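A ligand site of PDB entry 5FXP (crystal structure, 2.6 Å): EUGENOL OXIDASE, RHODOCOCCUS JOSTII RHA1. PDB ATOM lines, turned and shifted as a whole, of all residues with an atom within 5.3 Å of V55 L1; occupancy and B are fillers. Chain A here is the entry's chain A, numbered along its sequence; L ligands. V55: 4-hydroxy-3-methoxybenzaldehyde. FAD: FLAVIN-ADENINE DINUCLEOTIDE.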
ATOM      1  N   ASN A  89      17.778 -14.643  35.052  1.00  0.00           N
ATOM      2  CA  ASN A  89      18.658 -15.585  34.398  1.00  0.00           C
ATOM      3  C   ASN A  89      18.852 -15.144  32.973  1.00  0.00           C
ATOM      4  O   ASN A  89      17.902 -14.747  32.322  1.00  0.00           O
ATOM      5  CB  ASN A  89      18.045 -16.981  34.414  1.00  0.00           C
ATOM      6  CG  ASN A  89      17.878 -17.535  35.814  1.00  0.00           C
ATOM      7  OD1 ASN A  89      18.562 -17.136  36.763  1.00  0.00           O
ATOM      8  ND2 ASN A  89      16.962 -18.481  35.958  1.00  0.00           N
ATOM      9  N   GLY A  90      20.079 -15.166  32.505  1.00  0.00           N
ATOM     10  CA  GLY A  90      20.422 -14.554  31.230  1.00  0.00           C
ATOM     11  C   GLY A  90      21.093 -13.221  31.469  1.00  0.00           C
ATOM     12  O   GLY A  90      21.777 -12.716  30.580  1.00  0.00           O
ATOM     13  N   TYR A  91      20.892 -12.645  32.655  1.00  0.00           N
ATOM     14  CA  TYR A  91      21.519 -11.389  33.004  1.00  0.00           C
ATOM     15  C   TYR A  91      22.300 -11.415  34.315  1.00  0.00           C
ATOM     16  O   TYR A  91      22.762 -10.374  34.764  1.00  0.00           O
ATOM     17  CB  TYR A  91      20.450 -10.320  33.025  1.00  0.00           C
ATOM     18  CG  TYR A  91      19.809 -10.079  31.670  1.00  0.00           C
ATOM     19  CD1 TYR A  91      20.561  -9.672  30.572  1.00  0.00           C
ATOM     20  CD2 TYR A  91      18.434 -10.224  31.509  1.00  0.00           C
ATOM     21  CE1 TYR A  91      19.945  -9.418  29.349  1.00  0.00           C
ATOM     22  CE2 TYR A  91      17.821  -9.985  30.304  1.00  0.00           C
ATOM     23  CZ  TYR A  91      18.567  -9.577  29.214  1.00  0.00           C
ATOM     24  OH  TYR A  91      17.914  -9.347  28.015  1.00  0.00           O
ATOM     25  N   ASP A 151       8.055 -14.768  28.969  1.00  0.00           N
ATOM     26  CA  ASP A 151       8.216 -16.189  28.592  1.00  0.00           C
ATOM     27  C   ASP A 151       8.269 -17.135  29.752  1.00  0.00           C
ATOM     28  O   ASP A 151       7.849 -18.274  29.617  1.00  0.00           O
ATOM     29  CB  ASP A 151       9.493 -16.384  27.760  1.00  0.00           C
ATOM     30  CG  ASP A 151       9.360 -15.845  26.306  1.00  0.00           C
ATOM     31  OD1 ASP A 151       8.224 -15.479  25.913  1.00  0.00           O
ATOM     32  OD2 ASP A 151      10.375 -15.811  25.552  1.00  0.00           O
ATOM     33  N   VAL A 166       9.936  -7.166  29.395  1.00  0.00           N
ATOM     34  CA  VAL A 166       8.832  -7.067  28.459  1.00  0.00           C
ATOM     35  C   VAL A 166       8.009  -8.333  28.466  1.00  0.00           C
ATOM     36  O   VAL A 166       8.472  -9.396  28.857  1.00  0.00           O
ATOM     37  CB  VAL A 166       9.314  -6.767  27.020  1.00  0.00           C
ATOM     38  CG1 VAL A 166       9.998  -5.431  27.023  1.00  0.00           C
ATOM     39  CG2 VAL A 166      10.280  -7.827  26.506  1.00  0.00           C
ATOM     40  N   TYR A 168       3.987  -9.728  26.398  1.00  0.00           N
ATOM     41  CA  TYR A 168       3.485  -9.951  25.027  1.00  0.00           C
ATOM     42  C   TYR A 168       2.015  -9.638  24.760  1.00  0.00           C
ATOM     43  O   TYR A 168       1.597  -9.712  23.607  1.00  0.00           O
ATOM     44  CB  TYR A 168       3.899 -11.355  24.526  1.00  0.00           C
ATOM     45  CG  TYR A 168       5.389 -11.574  24.701  1.00  0.00           C
ATOM     46  CD1 TYR A 168       6.303 -11.070  23.778  1.00  0.00           C
ATOM     47  CD2 TYR A 168       5.891 -12.212  25.827  1.00  0.00           C
ATOM     48  CE1 TYR A 168       7.679 -11.231  23.975  1.00  0.00           C
ATOM     49  CE2 TYR A 168       7.257 -12.359  26.027  1.00  0.00           C
ATOM     50  CZ  TYR A 168       8.148 -11.878  25.099  1.00  0.00           C
ATOM     51  OH  TYR A 168       9.498 -12.055  25.316  1.00  0.00           O
ATOM     52  N   MET A 282      15.991 -20.994  17.855  1.00  0.00           N
ATOM     53  CA  MET A 282      15.184 -20.635  19.039  1.00  0.00           C
ATOM     54  C   MET A 282      14.002 -21.590  19.158  1.00  0.00           C
ATOM     55  O   MET A 282      13.780 -22.125  20.231  1.00  0.00           O
ATOM     56  CB  MET A 282      14.751 -19.155  18.922  1.00  0.00           C
ATOM     57  CG  MET A 282      13.840 -18.558  19.985  1.00  0.00           C
ATOM     58  SD  MET A 282      14.506 -18.244  21.630  1.00  0.00           S
ATOM     59  CE  MET A 282      15.494 -16.775  21.412  1.00  0.00           C
ATOM     60  N   GLU A 378       9.401 -22.727  27.998  1.00  0.00           N
ATOM     61  CA  GLU A 378      10.668 -22.172  27.515  1.00  0.00           C
ATOM     62  C   GLU A 378      11.908 -22.615  28.290  1.00  0.00           C
ATOM     63  O   GLU A 378      12.994 -22.453  27.785  1.00  0.00           O
ATOM     64  CB  GLU A 378      10.580 -20.635  27.488  1.00  0.00           C
ATOM     65  CG  GLU A 378       9.722 -20.054  26.358  1.00  0.00           C
ATOM     66  CD  GLU A 378      10.503 -19.797  25.065  1.00  0.00           C
ATOM     67  OE1 GLU A 378      11.122 -18.694  24.923  1.00  0.00           O
ATOM     68  OE2 GLU A 378      10.497 -20.718  24.209  1.00  0.00           O
ATOM     69  N   HIS A 390      22.118 -19.715  28.969  1.00  0.00           N
ATOM     70  CA  HIS A 390      22.056 -18.624  27.997  1.00  0.00           C
ATOM     71  C   HIS A 390      22.512 -17.286  28.543  1.00  0.00           C
ATOM     72  O   HIS A 390      22.536 -17.014  29.726  1.00  0.00           O
ATOM     73  CB  HIS A 390      20.647 -18.499  27.364  1.00  0.00           C
ATOM     74  CG  HIS A 390      19.597 -17.957  28.281  1.00  0.00           C
ATOM     75  ND1 HIS A 390      19.263 -16.627  28.335  1.00  0.00           N
ATOM     76  CD2 HIS A 390      18.778 -18.575  29.173  1.00  0.00           C
ATOM     77  CE1 HIS A 390      18.303 -16.432  29.212  1.00  0.00           C
ATOM     78  NE2 HIS A 390      17.945 -17.610  29.716  1.00  0.00           N
ATOM     79  N   ILE A 391      22.918 -16.451  27.605  1.00  0.00           N
ATOM     80  CA  ILE A 391      23.092 -15.043  27.868  1.00  0.00           C
ATOM     81  C   ILE A 391      22.255 -14.223  26.869  1.00  0.00           C
ATOM     82  O   ILE A 391      22.012 -14.638  25.727  1.00  0.00           O
ATOM     83  CB  ILE A 391      24.570 -14.652  27.811  1.00  0.00           C
ATOM     84  CG1 ILE A 391      24.755 -13.262  28.428  1.00  0.00           C
ATOM     85  CG2 ILE A 391      25.091 -14.741  26.374  1.00  0.00           C
ATOM     86  CD1 ILE A 391      26.219 -12.850  28.532  1.00  0.00           C
ATOM     87  N   GLY A 392      21.799 -13.070  27.359  1.00  0.00           N
ATOM     88  CA  GLY A 392      21.053 -12.103  26.585  1.00  0.00           C
ATOM     89  C   GLY A 392      21.950 -10.986  26.082  1.00  0.00           C
ATOM     90  O   GLY A 392      22.524 -10.230  26.858  1.00  0.00           O
ATOM     91  N   SER A 394      21.061  -7.939  23.828  1.00  0.00           N
ATOM     92  CA  SER A 394      19.743  -7.380  23.565  1.00  0.00           C
ATOM     93  C   SER A 394      19.810  -5.989  22.979  1.00  0.00           C
ATOM     94  O   SER A 394      19.334  -5.043  23.593  1.00  0.00           O
ATOM     95  CB  SER A 394      18.954  -7.378  24.864  1.00  0.00           C
ATOM     96  OG  SER A 394      19.208  -8.567  25.563  1.00  0.00           O
ATOM     97  N   GLN A 425      15.233 -13.601  18.732  1.00  0.00           N
ATOM     98  CA  GLN A 425      13.833 -13.247  18.987  1.00  0.00           C
ATOM     99  C   GLN A 425      13.659 -11.739  18.926  1.00  0.00           C
ATOM    100  O   GLN A 425      13.978 -11.032  19.887  1.00  0.00           O
ATOM    101  CB  GLN A 425      13.372 -13.780  20.360  1.00  0.00           C
ATOM    102  CG  GLN A 425      12.013 -13.268  20.806  1.00  0.00           C
ATOM    103  CD  GLN A 425      11.320 -14.164  21.818  1.00  0.00           C
ATOM    104  OE1 GLN A 425      11.151 -15.344  21.592  1.00  0.00           O
ATOM    105  NE2 GLN A 425      10.863 -13.584  22.932  1.00  0.00           N
ATOM    106  N   ILE A 427      11.407  -8.792  19.376  1.00  0.00           N
ATOM    107  CA  ILE A 427      10.183  -8.451  20.125  1.00  0.00           C
ATOM    108  C   ILE A 427       9.803  -7.065  19.607  1.00  0.00           C
ATOM    109  O   ILE A 427      10.621  -6.170  19.655  1.00  0.00           O
ATOM    110  CB  ILE A 427      10.459  -8.451  21.638  1.00  0.00           C
ATOM    111  CG1 ILE A 427      11.206  -9.732  22.039  1.00  0.00           C
ATOM    112  CG2 ILE A 427       9.172  -8.232  22.417  1.00  0.00           C
ATOM    113  CD1 ILE A 427      11.726  -9.749  23.465  1.00  0.00           C
ATOM    114  N   VAL A 436      16.520  -9.630  20.879  1.00  0.00           N
ATOM    115  CA  VAL A 436      17.105 -10.546  21.825  1.00  0.00           C
ATOM    116  C   VAL A 436      17.849 -11.652  21.087  1.00  0.00           C
ATOM    117  O   VAL A 436      17.296 -12.387  20.271  1.00  0.00           O
ATOM    118  CB  VAL A 436      16.061 -11.108  22.788  1.00  0.00           C
ATOM    119  CG1 VAL A 436      16.687 -12.161  23.698  1.00  0.00           C
ATOM    120  CG2 VAL A 436      15.476  -9.961  23.598  1.00  0.00           C
ATOM    121  N   LEU A 438      19.876 -14.784  22.059  1.00  0.00           N
ATOM    122  CA  LEU A 438      20.190 -15.741  23.119  1.00  0.00           C
ATOM    123  C   LEU A 438      21.215 -16.695  22.614  1.00  0.00           C
ATOM    124  O   LEU A 438      20.965 -17.443  21.684  1.00  0.00           O
ATOM    125  CB  LEU A 438      18.975 -16.587  23.491  1.00  0.00           C
ATOM    126  CG  LEU A 438      17.912 -16.085  24.417  1.00  0.00           C
ATOM    127  CD1 LEU A 438      17.227 -17.298  25.049  1.00  0.00           C
ATOM    128  CD2 LEU A 438      18.500 -15.200  25.486  1.00  0.00           C
ATOM    129  N   TYR A 471      19.348  -2.572  25.384  1.00  0.00           N
ATOM    130  CA  TYR A 471      18.312  -2.128  26.344  1.00  0.00           C
ATOM    131  C   TYR A 471      18.508  -2.696  27.765  1.00  0.00           C
ATOM    132  O   TYR A 471      17.935  -2.190  28.731  1.00  0.00           O
ATOM    133  CB  TYR A 471      16.931  -2.460  25.824  1.00  0.00           C
ATOM    134  CG  TYR A 471      16.283  -3.691  26.425  1.00  0.00           C
ATOM    135  CD1 TYR A 471      16.543  -4.954  25.909  1.00  0.00           C
ATOM    136  CD2 TYR A 471      15.365  -3.589  27.452  1.00  0.00           C
ATOM    137  CE1 TYR A 471      15.912  -6.081  26.427  1.00  0.00           C
ATOM    138  CE2 TYR A 471      14.744  -4.711  27.978  1.00  0.00           C
ATOM    139  CZ  TYR A 471      15.017  -5.958  27.472  1.00  0.00           C
ATOM    140  OH  TYR A 471      14.389  -7.061  28.029  1.00  0.00           O
ATOM    141  N   ARG A 472      19.310  -3.757  27.880  1.00  0.00           N
ATOM    142  CA  ARG A 472      19.412  -4.548  29.100  1.00  0.00           C
ATOM    143  C   ARG A 472      20.598  -5.451  28.928  1.00  0.00           C
ATOM    144  O   ARG A 472      20.835  -5.935  27.828  1.00  0.00           O
ATOM    145  CB  ARG A 472      18.135  -5.372  29.276  1.00  0.00           C
ATOM    146  CG  ARG A 472      17.969  -6.105  30.582  1.00  0.00           C
ATOM    147  CD  ARG A 472      16.524  -6.537  30.690  1.00  0.00           C
ATOM    148  NE  ARG A 472      16.260  -7.404  31.846  1.00  0.00           N
ATOM    149  CZ  ARG A 472      15.210  -8.213  31.968  1.00  0.00           C
ATOM    150  NH1 ARG A 472      14.281  -8.301  31.017  1.00  0.00           N
ATOM    151  NH2 ARG A 472      15.089  -8.958  33.058  1.00  0.00           N
HETATM  152  CAI V55 L   1      13.622 -12.944  26.231  1.00  0.00           C
HETATM  153  CAG V55 L   1      14.801 -13.058  26.965  1.00  0.00           C
HETATM  154  CAK V55 L   1      15.401 -11.910  27.511  1.00  0.00           C
HETATM  155  CAJ V55 L   1      14.816 -10.646  27.330  1.00  0.00           C
HETATM  156  CAF V55 L   1      13.634 -10.543  26.608  1.00  0.00           C
HETATM  157  OAB V55 L   1      13.462 -15.186  25.664  1.00  0.00           O
HETATM  158  CAE V55 L   1      13.047 -11.676  26.072  1.00  0.00           C
HETATM  159  CAD V55 L   1      12.969 -14.052  25.685  1.00  0.00           C
HETATM  160  CAA V55 L   1      17.544 -12.864  27.830  1.00  0.00           C
HETATM  161  OAH V55 L   1      16.549 -11.941  28.258  1.00  0.00           O
HETATM  162  OAC V55 L   1      15.430  -9.542  27.854  1.00  0.00           O
HETATM  163  PA  FAD L   2      14.887 -10.141  39.864  1.00  0.00           P
HETATM  164  O1A FAD L   2      15.994 -11.100  39.546  1.00  0.00           O
HETATM  165  O2A FAD L   2      14.278 -10.282  41.256  1.00  0.00           O
HETATM  166  O5B FAD L   2      15.343  -8.612  39.696  1.00  0.00           O
HETATM  167  C5B FAD L   2      15.823  -8.066  38.462  1.00  0.00           C
HETATM  168  C4B FAD L   2      16.698  -6.871  38.787  1.00  0.00           C
HETATM  169  O4B FAD L   2      15.889  -5.743  39.134  1.00  0.00           O
HETATM  170  C3B FAD L   2      17.577  -7.120  40.006  1.00  0.00           C
HETATM  171  O3B FAD L   2      18.773  -7.772  39.652  1.00  0.00           O
HETATM  172  C2B FAD L   2      17.823  -5.756  40.519  1.00  0.00           C
HETATM  173  O2B FAD L   2      18.822  -5.193  39.707  1.00  0.00           O
HETATM  174  C1B FAD L   2      16.494  -5.098  40.258  1.00  0.00           C
HETATM  175  N9A FAD L   2      15.597  -5.280  41.405  1.00  0.00           N
HETATM  176  C8A FAD L   2      14.784  -6.309  41.644  1.00  0.00           C
HETATM  177  N7A FAD L   2      14.058  -6.140  42.769  1.00  0.00           N
HETATM  178  C5A FAD L   2      14.416  -4.974  43.266  1.00  0.00           C
HETATM  179  C6A FAD L   2      14.053  -4.213  44.452  1.00  0.00           C
HETATM  180  N6A FAD L   2      13.140  -4.724  45.281  1.00  0.00           N
HETATM  181  N1A FAD L   2      14.652  -3.040  44.650  1.00  0.00           N
HETATM  182  C2A FAD L   2      15.569  -2.536  43.785  1.00  0.00           C
HETATM  183  N3A FAD L   2      15.954  -3.178  42.682  1.00  0.00           N
HETATM  184  C4A FAD L   2      15.422  -4.400  42.375  1.00  0.00           C
HETATM  185  N1  FAD L   2      12.754 -11.420  30.551  1.00  0.00           N
HETATM  186  C2  FAD L   2      11.706 -10.703  30.115  1.00  0.00           C
HETATM  187  O2  FAD L   2      11.527  -9.567  30.575  1.00  0.00           O
HETATM  188  N3  FAD L   2      10.825 -11.134  29.196  1.00  0.00           N
HETATM  189  C4  FAD L   2      10.935 -12.349  28.644  1.00  0.00           C
HETATM  190  O4  FAD L   2      10.086 -12.698  27.809  1.00  0.00           O
HETATM  191  C4X FAD L   2      12.063 -13.224  29.084  1.00  0.00           C
HETATM  192  N5  FAD L   2      12.250 -14.437  28.562  1.00  0.00           N
HETATM  193  C5X FAD L   2      13.294 -15.181  28.972  1.00  0.00           C
HETATM  194  C6  FAD L   2      13.442 -16.419  28.417  1.00  0.00           C
HETATM  195  C7  FAD L   2      14.496 -17.239  28.808  1.00  0.00           C
HETATM  196  C7M FAD L   2      14.628 -18.598  28.176  1.00  0.00           C
HETATM  197  C8  FAD L   2      15.467 -16.780  29.833  1.00  0.00           C
HETATM  198  C8M FAD L   2      16.668 -17.651  30.217  1.00  0.00           C
HETATM  199  C9  FAD L   2      15.300 -15.535  30.382  1.00  0.00           C
HETATM  200  C9A FAD L   2      14.258 -14.700  30.000  1.00  0.00           C
HETATM  201  N10 FAD L   2      14.077 -13.408  30.557  1.00  0.00           N
HETATM  202  C10 FAD L   2      12.987 -12.660  30.089  1.00  0.00           C
HETATM  203  C1' FAD L   2      14.984 -12.807  31.568  1.00  0.00           C
HETATM  204  C2' FAD L   2      14.570 -12.958  33.060  1.00  0.00           C
HETATM  205  O2' FAD L   2      14.584 -14.307  33.481  1.00  0.00           O
HETATM  206  C3' FAD L   2      13.204 -12.350  33.456  1.00  0.00           C
HETATM  207  O3' FAD L   2      13.223 -10.960  33.113  1.00  0.00           O
HETATM  208  C4' FAD L   2      12.894 -12.462  34.954  1.00  0.00           C
HETATM  209  O4' FAD L   2      11.510 -12.128  35.228  1.00  0.00           O
HETATM  210  C5' FAD L   2      13.767 -11.544  35.801  1.00  0.00           C
HETATM  211  O5' FAD L   2      13.956 -12.073  37.129  1.00  0.00           O
HETATM  212  P   FAD L   2      13.002 -11.575  38.305  1.00  0.00           P
HETATM  213  O1P FAD L   2      13.076 -12.547  39.446  1.00  0.00           O
HETATM  214  O2P FAD L   2      11.652 -11.303  37.703  1.00  0.00           O
HETATM  215  O3P FAD L   2      13.769 -10.198  38.666  1.00  0.00           O
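The side-chain carboxylate (OD2) of Asp 151 sits close to an oxygen (OAB) of V55 L1, at 3.2 Å. OH of Tyr 168 touches CAE of V55 L1, at 3.6 Å. His 390 touches V55 L1 (CE1 to CAA, 3.9 Å). Gly 392 touches V55 L1 (CA to CAA, 3.8 Å). Gln 425 touches V55 L1. Ile 427 touches V55 L1. CG2 of Val 436 touches CAF of V55 L1, 3.6 Å away. Leu 438 touches V55 L1 (CD2 to CAA, 3.4 Å). Arg 472 touches V55 L1 (NH1 to OAC, 3.6 Å). Of the 18 residues printed, 11 come within 4 Å of V55 L1. Along chain A the residues within 4 Å of V55 L1 span positions 91 to 472. The nearest printed residue that does not touch V55 L1 is Glu 378 (4.3 Å).
An oxygen (O3') of FAD L2 lies within hydrogen-bond range of the guanidinium group (NH2) of Arg 472 (2.7 Å). The backbone carbonyl oxygen (O) of Val 166 sits at hydrogen-bond distance from a nitrogen (N3) of FAD L2 (2.9 Å). OH of Tyr 168 sits at hydrogen-bond distance from O4 of FAD L2 (2.6 Å). The side-chain hydroxyl (OH) of Tyr 91 is in hydrogen-bond range of an oxygen (OAC) of V55 L1, at 2.5 Å. The side-chain hydroxyl (OH) of Tyr 471 is in hydrogen-bond range of an oxygen (OAC) of V55 L1, at 2.7 Å. NE2 of His 390 is bonded to C8M of FAD L2 (1.4 Å). The backbone NH of Val 166 lies within hydrogen-bond range of an oxygen (O2) of FAD L2, at 3.1 Å. N of Asp 151 is in hydrogen-bond range of O4 of FAD L2 (3.1 Å).
The backbone NH (N) of Tyr 471 lies within hydrogen-bond range of the backbone carbonyl oxygen (O) of Ser 394. The side-chain amide nitrogen (NE2) of Gln 425 lies within hydrogen-bond range of the side-chain carboxylate (OD2) of Asp 151 (3.5 Å). NE2 of Gln 425 is in hydrogen-bond range of OH of Tyr 168. The side-chain hydroxyl (OG) of Ser 394 sits at hydrogen-bond distance from the side-chain hydroxyl (OH) of Tyr 91, 2.9 Å away. The backbone carbonyl oxygen (O) of Gly 90 lies within hydrogen-bond range of the backbone NH (N) of Gly 392 (3.2 Å). The backbone carbonyl oxygen of Val 436 sits at hydrogen-bond distance from the backbone NH of Gln 425, 2.8 Å away. OH of Tyr 471 lies within hydrogen-bond range of NH1 of Arg 472 (3.2 Å).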
